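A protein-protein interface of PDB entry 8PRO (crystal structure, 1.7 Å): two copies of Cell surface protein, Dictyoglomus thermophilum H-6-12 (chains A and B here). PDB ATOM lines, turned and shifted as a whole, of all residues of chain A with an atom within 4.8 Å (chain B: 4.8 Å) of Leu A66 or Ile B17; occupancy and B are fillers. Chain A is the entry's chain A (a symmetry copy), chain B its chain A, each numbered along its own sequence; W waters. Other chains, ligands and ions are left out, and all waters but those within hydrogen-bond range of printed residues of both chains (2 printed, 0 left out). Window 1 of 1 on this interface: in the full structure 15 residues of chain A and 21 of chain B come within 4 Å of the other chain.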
ATOM      1  N   TYR A  58      18.162 -24.007 -15.485  1.00  0.00           N
ATOM      2  CA  TYR A  58      18.822 -24.873 -16.450  1.00  0.00           C
ATOM      3  C   TYR A  58      20.091 -25.420 -15.834  1.00  0.00           C
ATOM      4  O   TYR A  58      20.871 -24.666 -15.244  1.00  0.00           O
ATOM      5  CB  TYR A  58      19.171 -24.120 -17.732  1.00  0.00           C
ATOM      6  CG  TYR A  58      18.004 -23.414 -18.365  1.00  0.00           C
ATOM      7  CD1 TYR A  58      17.152 -24.087 -19.241  1.00  0.00           C
ATOM      8  CD2 TYR A  58      17.763 -22.076 -18.100  1.00  0.00           C
ATOM      9  CE1 TYR A  58      16.078 -23.446 -19.829  1.00  0.00           C
ATOM     10  CE2 TYR A  58      16.685 -21.420 -18.684  1.00  0.00           C
ATOM     11  CZ  TYR A  58      15.855 -22.110 -19.545  1.00  0.00           C
ATOM     12  OH  TYR A  58      14.796 -21.451 -20.122  1.00  0.00           O
ATOM     13  N   VAL A  59      20.314 -26.713 -15.997  1.00  0.00           N
ATOM     14  CA  VAL A  59      21.529 -27.303 -15.456  1.00  0.00           C
ATOM     15  C   VAL A  59      21.869 -28.538 -16.273  1.00  0.00           C
ATOM     16  O   VAL A  59      20.983 -29.264 -16.735  1.00  0.00           O
ATOM     17  CB  VAL A  59      21.368 -27.579 -13.945  1.00  0.00           C
ATOM     18  CG1 VAL A  59      20.466 -28.754 -13.687  1.00  0.00           C
ATOM     19  CG2 VAL A  59      22.729 -27.734 -13.288  1.00  0.00           C
ATOM     20  N   GLY A  60      23.161 -28.739 -16.500  1.00  0.00           N
ATOM     21  CA  GLY A  60      23.626 -29.934 -17.163  1.00  0.00           C
ATOM     22  C   GLY A  60      23.851 -31.042 -16.156  1.00  0.00           C
ATOM     23  O   GLY A  60      24.054 -30.804 -14.968  1.00  0.00           O
ATOM     24  N   HIS A  64      24.208 -36.741 -19.560  1.00  0.00           N
ATOM     25  CA  HIS A  64      24.338 -36.182 -20.911  1.00  0.00           C
ATOM     26  C   HIS A  64      23.174 -35.267 -21.273  1.00  0.00           C
ATOM     27  O   HIS A  64      23.107 -34.799 -22.418  1.00  0.00           O
ATOM     28  CB  HIS A  64      24.481 -37.262 -21.991  1.00  0.00           C
ATOM     29  CG  HIS A  64      25.670 -38.155 -21.807  1.00  0.00           C
ATOM     30  ND1 HIS A  64      26.113 -39.013 -22.791  1.00  0.00           N
ATOM     31  CD2 HIS A  64      26.505 -38.327 -20.755  1.00  0.00           C
ATOM     32  CE1 HIS A  64      27.171 -39.672 -22.355  1.00  0.00           C
ATOM     33  NE2 HIS A  64      27.429 -39.278 -21.120  1.00  0.00           N
ATOM     34  N   TYR A  65      22.272 -34.977 -20.342  1.00  0.00           N
ATOM     35  CA  TYR A  65      21.114 -34.129 -20.597  1.00  0.00           C
ATOM     36  C   TYR A  65      21.342 -32.718 -20.072  1.00  0.00           C
ATOM     37  O   TYR A  65      21.973 -32.527 -19.032  1.00  0.00           O
ATOM     38  CB  TYR A  65      19.868 -34.715 -19.931  1.00  0.00           C
ATOM     39  CG  TYR A  65      19.230 -35.853 -20.695  1.00  0.00           C
ATOM     40  CD1 TYR A  65      18.481 -35.611 -21.839  1.00  0.00           C
ATOM     41  CD2 TYR A  65      19.409 -37.172 -20.296  1.00  0.00           C
ATOM     42  CE1 TYR A  65      17.895 -36.647 -22.538  1.00  0.00           C
ATOM     43  CE2 TYR A  65      18.840 -38.214 -20.998  1.00  0.00           C
ATOM     44  CZ  TYR A  65      18.087 -37.944 -22.124  1.00  0.00           C
ATOM     45  OH  TYR A  65      17.511 -38.976 -22.829  1.00  0.00           O
ATOM     46  N   LEU A  66      20.818 -31.732 -20.791  1.00  0.00           N
ATOM     47  CA  LEU A  66      20.597 -30.405 -20.241  1.00  0.00           C
ATOM     48  C   LEU A  66      19.155 -30.373 -19.760  1.00  0.00           C
ATOM     49  O   LEU A  66      18.234 -30.608 -20.546  1.00  0.00           O
ATOM     50  CB  LEU A  66      20.843 -29.300 -21.264  1.00  0.00           C
ATOM     51  CG  LEU A  66      20.471 -27.916 -20.729  1.00  0.00           C
ATOM     52  CD1 LEU A  66      21.532 -27.402 -19.791  1.00  0.00           C
ATOM     53  CD2 LEU A  66      20.253 -26.932 -21.859  1.00  0.00           C
ATOM     54  N   TYR A  67      18.966 -30.112 -18.473  1.00  0.00           N
ATOM     55  CA  TYR A  67      17.644 -30.071 -17.868  1.00  0.00           C
ATOM     56  C   TYR A  67      17.125 -28.644 -17.817  1.00  0.00           C
ATOM     57  O   TYR A  67      17.881 -27.707 -17.547  1.00  0.00           O
ATOM     58  CB  TYR A  67      17.698 -30.637 -16.449  1.00  0.00           C
ATOM     59  CG  TYR A  67      17.813 -32.135 -16.411  1.00  0.00           C
ATOM     60  CD1 TYR A  67      19.052 -32.758 -16.497  1.00  0.00           C
ATOM     61  CD2 TYR A  67      16.681 -32.931 -16.320  1.00  0.00           C
ATOM     62  CE1 TYR A  67      19.156 -34.130 -16.471  1.00  0.00           C
ATOM     63  CE2 TYR A  67      16.774 -34.302 -16.301  1.00  0.00           C
ATOM     64  CZ  TYR A  67      18.016 -34.897 -16.377  1.00  0.00           C
ATOM     65  OH  TYR A  67      18.110 -36.267 -16.354  1.00  0.00           O
ATOM     66  N   ALA A  68      15.829 -28.487 -18.074  1.00  0.00           N
ATOM     67  CA  ALA A  68      15.105 -27.255 -17.794  1.00  0.00           C
ATOM     68  C   ALA A  68      14.041 -27.591 -16.762  1.00  0.00           C
ATOM     69  O   ALA A  68      13.175 -28.432 -17.023  1.00  0.00           O
ATOM     70  CB  ALA A  68      14.476 -26.684 -19.065  1.00  0.00           C
ATOM     71  N   TRP A  77      11.626 -29.531 -19.670  1.00  0.00           N
ATOM     72  CA  TRP A  77      12.087 -30.399 -20.746  1.00  0.00           C
ATOM     73  C   TRP A  77      13.517 -30.808 -20.437  1.00  0.00           C
ATOM     74  O   TRP A  77      14.166 -30.252 -19.547  1.00  0.00           O
ATOM     75  CB  TRP A  77      11.987 -29.734 -22.132  1.00  0.00           C
ATOM     76  CG  TRP A  77      12.519 -28.309 -22.256  1.00  0.00           C
ATOM     77  CD1 TRP A  77      11.768 -27.170 -22.363  1.00  0.00           C
ATOM     78  CD2 TRP A  77      13.891 -27.887 -22.333  1.00  0.00           C
ATOM     79  NE1 TRP A  77      12.580 -26.075 -22.471  1.00  0.00           N
ATOM     80  CE2 TRP A  77      13.888 -26.484 -22.465  1.00  0.00           C
ATOM     81  CE3 TRP A  77      15.118 -28.554 -22.301  1.00  0.00           C
ATOM     82  CZ2 TRP A  77      15.066 -25.738 -22.562  1.00  0.00           C
ATOM     83  CZ3 TRP A  77      16.285 -27.814 -22.400  1.00  0.00           C
ATOM     84  CH2 TRP A  77      16.252 -26.423 -22.530  1.00  0.00           C
ATOM     85  N   LYS A  78      13.988 -31.816 -21.168  1.00  0.00           N
ATOM     86  CA  LYS A  78      15.379 -32.230 -21.140  1.00  0.00           C
ATOM     87  C   LYS A  78      15.866 -32.350 -22.574  1.00  0.00           C
ATOM     88  O   LYS A  78      15.125 -32.796 -23.452  1.00  0.00           O
ATOM     89  CB  LYS A  78      15.548 -33.554 -20.387  1.00  0.00           C
ATOM     90  CG  LYS A  78      14.655 -34.651 -20.934  1.00  0.00           C
ATOM     91  CD  LYS A  78      15.024 -36.044 -20.440  1.00  0.00           C
ATOM     92  CE  LYS A  78      15.267 -36.085 -18.952  1.00  0.00           C
ATOM     93  NZ  LYS A  78      16.311 -37.094 -18.614  1.00  0.00           N
ATOM     94  N   PHE A  79      17.099 -31.915 -22.815  1.00  0.00           N
ATOM     95  CA  PHE A  79      17.677 -31.897 -24.149  1.00  0.00           C
ATOM     96  C   PHE A  79      18.900 -32.801 -24.193  1.00  0.00           C
ATOM     97  O   PHE A  79      19.810 -32.666 -23.367  1.00  0.00           O
ATOM     98  CB  PHE A  79      18.046 -30.471 -24.568  1.00  0.00           C
ATOM     99  CG  PHE A  79      18.763 -30.399 -25.881  1.00  0.00           C
ATOM    100  CD1 PHE A  79      20.145 -30.517 -25.946  1.00  0.00           C
ATOM    101  CD2 PHE A  79      18.055 -30.251 -27.052  1.00  0.00           C
ATOM    102  CE1 PHE A  79      20.800 -30.463 -27.152  1.00  0.00           C
ATOM    103  CE2 PHE A  79      18.709 -30.200 -28.263  1.00  0.00           C
ATOM    104  CZ  PHE A  79      20.081 -30.306 -28.310  1.00  0.00           C
ATOM    105  N   VAL B   5      27.468 -32.961 -19.872  1.00  0.00           N
ATOM    106  CA  VAL B   5      27.376 -31.512 -19.924  1.00  0.00           C
ATOM    107  C   VAL B   5      27.971 -31.004 -18.615  1.00  0.00           C
ATOM    108  O   VAL B   5      27.269 -30.903 -17.601  1.00  0.00           O
ATOM    109  CB  VAL B   5      25.917 -31.049 -20.106  1.00  0.00           C
ATOM    110  CG1 VAL B   5      25.807 -29.521 -20.013  1.00  0.00           C
ATOM    111  CG2 VAL B   5      25.340 -31.565 -21.421  1.00  0.00           C
ATOM    112  N   PRO B   9      25.478 -23.487 -18.184  1.00  0.00           N
ATOM    113  CA  PRO B   9      24.796 -22.749 -19.250  1.00  0.00           C
ATOM    114  C   PRO B   9      24.828 -21.246 -19.040  1.00  0.00           C
ATOM    115  O   PRO B   9      24.890 -20.739 -17.916  1.00  0.00           O
ATOM    116  CB  PRO B   9      23.358 -23.283 -19.201  1.00  0.00           C
ATOM    117  CG  PRO B   9      23.232 -24.034 -17.926  1.00  0.00           C
ATOM    118  CD  PRO B   9      24.605 -24.454 -17.501  1.00  0.00           C
ATOM    119  N   ALA B  10      24.801 -20.520 -20.154  1.00  0.00           N
ATOM    120  CA  ALA B  10      24.596 -19.079 -20.129  1.00  0.00           C
ATOM    121  C   ALA B  10      23.326 -18.782 -20.908  1.00  0.00           C
ATOM    122  O   ALA B  10      22.981 -19.506 -21.844  1.00  0.00           O
ATOM    123  CB  ALA B  10      25.780 -18.302 -20.723  1.00  0.00           C
ATOM    124  N   ILE B  11      22.624 -17.730 -20.506  1.00  0.00           N
ATOM    125  CA  ILE B  11      21.317 -17.388 -21.060  1.00  0.00           C
ATOM    126  C   ILE B  11      21.458 -16.085 -21.829  1.00  0.00           C
ATOM    127  O   ILE B  11      21.929 -15.083 -21.277  1.00  0.00           O
ATOM    128  CB  ILE B  11      20.254 -17.239 -19.959  1.00  0.00           C
ATOM    129  CG1 ILE B  11      20.100 -18.514 -19.114  1.00  0.00           C
ATOM    130  CG2 ILE B  11      18.915 -16.870 -20.564  1.00  0.00           C
ATOM    131  CD1 ILE B  11      20.114 -19.781 -19.893  1.00  0.00           C
ATOM    132  N   GLY B  15      16.569 -15.384 -24.216  1.00  0.00           N
ATOM    133  CA  GLY B  15      16.292 -16.620 -23.529  1.00  0.00           C
ATOM    134  C   GLY B  15      17.020 -17.826 -24.067  1.00  0.00           C
ATOM    135  O   GLY B  15      16.902 -18.907 -23.481  1.00  0.00           O
ATOM    136  N   THR B  16      17.739 -17.689 -25.179  1.00  0.00           N
ATOM    137  CA  THR B  16      18.517 -18.806 -25.703  1.00  0.00           C
ATOM    138  C   THR B  16      19.494 -19.305 -24.648  1.00  0.00           C
ATOM    139  O   THR B  16      20.116 -18.516 -23.933  1.00  0.00           O
ATOM    140  CB  THR B  16      19.279 -18.385 -26.956  1.00  0.00           C
ATOM    141  OG1 THR B  16      18.357 -17.822 -27.904  1.00  0.00           O
ATOM    142  CG2 THR B  16      19.987 -19.576 -27.569  1.00  0.00           C
ATOM    143  N   ILE B  17      19.619 -20.621 -24.551  1.00  0.00           N
ATOM    144  CA  ILE B  17      20.492 -21.269 -23.577  1.00  0.00           C
ATOM    145  C   ILE B  17      21.693 -21.808 -24.336  1.00  0.00           C
ATOM    146  O   ILE B  17      21.543 -22.588 -25.289  1.00  0.00           O
ATOM    147  CB  ILE B  17      19.767 -22.386 -22.812  1.00  0.00           C
ATOM    148  CG1 ILE B  17      18.479 -21.850 -22.184  1.00  0.00           C
ATOM    149  CG2 ILE B  17      20.675 -22.979 -21.728  1.00  0.00           C
ATOM    150  CD1 ILE B  17      17.224 -22.252 -22.928  1.00  0.00           C
ATOM    151  N   TYR B  18      22.882 -21.386 -23.925  1.00  0.00           N
ATOM    152  CA  TYR B  18      24.115 -21.830 -24.554  1.00  0.00           C
ATOM    153  C   TYR B  18      24.876 -22.687 -23.566  1.00  0.00           C
ATOM    154  O   TYR B  18      25.030 -22.302 -22.403  1.00  0.00           O
ATOM    155  CB  TYR B  18      24.987 -20.651 -24.968  1.00  0.00           C
ATOM    156  CG  TYR B  18      24.295 -19.643 -25.839  1.00  0.00           C
ATOM    157  CD1 TYR B  18      24.243 -19.802 -27.216  1.00  0.00           C
ATOM    158  CD2 TYR B  18      23.687 -18.541 -25.276  1.00  0.00           C
ATOM    159  CE1 TYR B  18      23.593 -18.861 -28.021  1.00  0.00           C
ATOM    160  CE2 TYR B  18      23.035 -17.597 -26.067  1.00  0.00           C
ATOM    161  CZ  TYR B  18      22.996 -17.765 -27.435  1.00  0.00           C
ATOM    162  OH  TYR B  18      22.357 -16.817 -28.216  1.00  0.00           O
ATOM    163  N   VAL B  19      25.370 -23.824 -24.030  1.00  0.00           N
ATOM    164  CA  VAL B  19      26.096 -24.710 -23.125  1.00  0.00           C
ATOM    165  C   VAL B  19      27.026 -25.583 -23.948  1.00  0.00           C
ATOM    166  O   VAL B  19      26.716 -25.965 -25.083  1.00  0.00           O
ATOM    167  CB  VAL B  19      25.115 -25.531 -22.252  1.00  0.00           C
ATOM    168  CG1 VAL B  19      24.427 -26.647 -23.058  1.00  0.00           C
ATOM    169  CG2 VAL B  19      25.817 -26.053 -21.003  1.00  0.00           C
ATOM    170  N   TYR B  27      26.267 -25.832 -27.878  1.00  0.00           N
ATOM    171  CA  TYR B  27      24.854 -25.873 -28.236  1.00  0.00           C
ATOM    172  C   TYR B  27      24.195 -24.529 -27.964  1.00  0.00           C
ATOM    173  O   TYR B  27      24.493 -23.878 -26.961  1.00  0.00           O
ATOM    174  CB  TYR B  27      24.115 -26.939 -27.429  1.00  0.00           C
ATOM    175  CG  TYR B  27      24.445 -28.338 -27.865  1.00  0.00           C
ATOM    176  CD1 TYR B  27      25.539 -29.002 -27.328  1.00  0.00           C
ATOM    177  CD2 TYR B  27      23.674 -28.993 -28.814  1.00  0.00           C
ATOM    178  CE1 TYR B  27      25.861 -30.281 -27.728  1.00  0.00           C
ATOM    179  CE2 TYR B  27      23.993 -30.281 -29.223  1.00  0.00           C
ATOM    180  CZ  TYR B  27      25.087 -30.917 -28.672  1.00  0.00           C
ATOM    181  OH  TYR B  27      25.416 -32.199 -29.062  1.00  0.00           O
ATOM    182  N   ALA B  28      23.282 -24.133 -28.851  1.00  0.00           N
ATOM    183  CA  ALA B  28      22.357 -23.031 -28.598  1.00  0.00           C
ATOM    184  C   ALA B  28      20.963 -23.623 -28.635  1.00  0.00           C
ATOM    185  O   ALA B  28      20.562 -24.191 -29.652  1.00  0.00           O
ATOM    186  CB  ALA B  28      22.494 -21.912 -29.632  1.00  0.00           C
ATOM    187  N   ILE B  29      20.244 -23.525 -27.521  1.00  0.00           N
ATOM    188  CA  ILE B  29      18.964 -24.201 -27.351  1.00  0.00           C
ATOM    189  C   ILE B  29      17.890 -23.141 -27.139  1.00  0.00           C
ATOM    190  O   ILE B  29      18.054 -22.239 -26.310  1.00  0.00           O
ATOM    191  CB  ILE B  29      19.025 -25.189 -26.175  1.00  0.00           C
ATOM    192  CG1 ILE B  29      20.087 -26.254 -26.471  1.00  0.00           C
ATOM    193  CG2 ILE B  29      17.671 -25.853 -25.929  1.00  0.00           C
ATOM    194  CD1 ILE B  29      20.788 -26.785 -25.275  1.00  0.00           C
ATOM    195  N   ASN B  30      16.796 -23.248 -27.887  1.00  0.00           N
ATOM    196  CA  ASN B  30      15.692 -22.324 -27.688  1.00  0.00           C
ATOM    197  C   ASN B  30      14.999 -22.627 -26.361  1.00  0.00           C
ATOM    198  O   ASN B  30      15.043 -23.759 -25.872  1.00  0.00           O
ATOM    199  CB  ASN B  30      14.698 -22.444 -28.836  1.00  0.00           C
ATOM    200  CG  ASN B  30      15.256 -21.925 -30.130  1.00  0.00           C
ATOM    201  OD1 ASN B  30      15.603 -20.744 -30.251  1.00  0.00           O
ATOM    202  ND2 ASN B  30      15.341 -22.806 -31.121  1.00  0.00           N
ATOM    203  N   PRO B  31      14.342 -21.630 -25.764  1.00  0.00           N
ATOM    204  CA  PRO B  31      13.673 -21.863 -24.480  1.00  0.00           C
ATOM    205  C   PRO B  31      12.617 -22.947 -24.536  1.00  0.00           C
ATOM    206  O   PRO B  31      12.262 -23.481 -23.482  1.00  0.00           O
ATOM    207  CB  PRO B  31      13.060 -20.495 -24.150  1.00  0.00           C
ATOM    208  CG  PRO B  31      13.903 -19.535 -24.878  1.00  0.00           C
ATOM    209  CD  PRO B  31      14.292 -20.211 -26.150  1.00  0.00           C
HETATM  210  O   HOH W   1      15.451 -18.960 -21.031  1.00  0.00           O
HETATM  211  O   HOH W   2      12.556 -22.499 -20.979  1.00  0.00           O
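No position is printed for both chains.
Of the 11 pairs that touch across the chains among the printed residues, none has its exchanged pair printed and touching as well.
Among the printed residues, pairs that only touch across the chains: Leu A66 with Ile B29 (3.5 Å), Tyr A58 with Ile B17 (3.5 Å), Gly A60 with Val B5 (3.6 Å), Tyr A58 with Pro B9 (3.6 Å), Phe A79 with Tyr B27 (3.6 Å), Trp A77 with Ile B29 (3.7 Å), Tyr A58 with Ile B11 (3.7 Å), Phe A79 with Ile B29 (3.8 Å), Trp A77 with Asn B30 (3.9 Å) and Leu A66 with Ile B17 (3.98 Å).
Printed residues of chain B that touch a printed residue of chain A: Val B5, Pro B9, Ile B11, Ile B17, Tyr B27, Ile B29, Asn B30 and Pro B31.
Of the 11 printed residues of chain A, 5 touch a printed residue of chain B.
Among the printed residues, no Asp or Glu carboxylate lies within 4 Å of a Lys or Arg side-chain nitrogen of the other chain.
Leu A66 touches two residues of chain B.
Ala A68 touches none of the printed residues of chain B.
Of the printed residues of chain B, Trp A77 touches Ile B29 (3.7 Å), Asn B30 (3.9 Å) and Pro B31 (2.8 Å).
Of the printed residues of chain B, Phe A79 touches Tyr B27 (3.6 Å) and Ile B29 (3.8 Å).
Of the printed residues of chain A, Pro B9 touches Tyr A58.
Printed residues of chain A within 4 Å of Ile B11: Tyr A58 (3.7 Å).
Ile B17 touches just these residues of chain A: Tyr A58 and Leu A66.
Printed residues of chain A within 4 Å of Ile B29: Leu A66 (3.5 Å), Trp A77 (3.7 Å) and Phe A79 (3.8 Å).
The nearest residue of chain B that does not touch Leu A66 is Pro B9 (4.2 Å).
The nearest residue of chain A that does not touch Ile B17 is Trp A77 (4.1 Å).
Water W2 lies within hydrogen-bond range of the side-chain hydroxyl (OH) of Tyr A58 and the backbone carbonyl oxygen (O) of Pro B31.
Water W1 bridges the side-chain hydroxyl of Tyr A58 (2.7 Å) and the backbone carbonyl oxygen of Gly B15 (2.8 Å).
The backbone NH (N) of Ile B29 is in hydrogen-bond range of the backbone carbonyl oxygen (O) of Ile B17, 2.7 Å away.
N of Tyr B27 lies within hydrogen-bond range of O of Val B19, at 2.8 Å.
The backbone carbonyl oxygen (O) of Leu A66 is in hydrogen-bond range of the backbone NH (N) of Phe A79.
The backbone NH of Ala A68 is in hydrogen-bond range of the backbone carbonyl oxygen of Trp A77 (2.8 Å).
The backbone carbonyl oxygen of Pro B31 sits at hydrogen-bond distance from the indole nitrogen of Trp A77.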
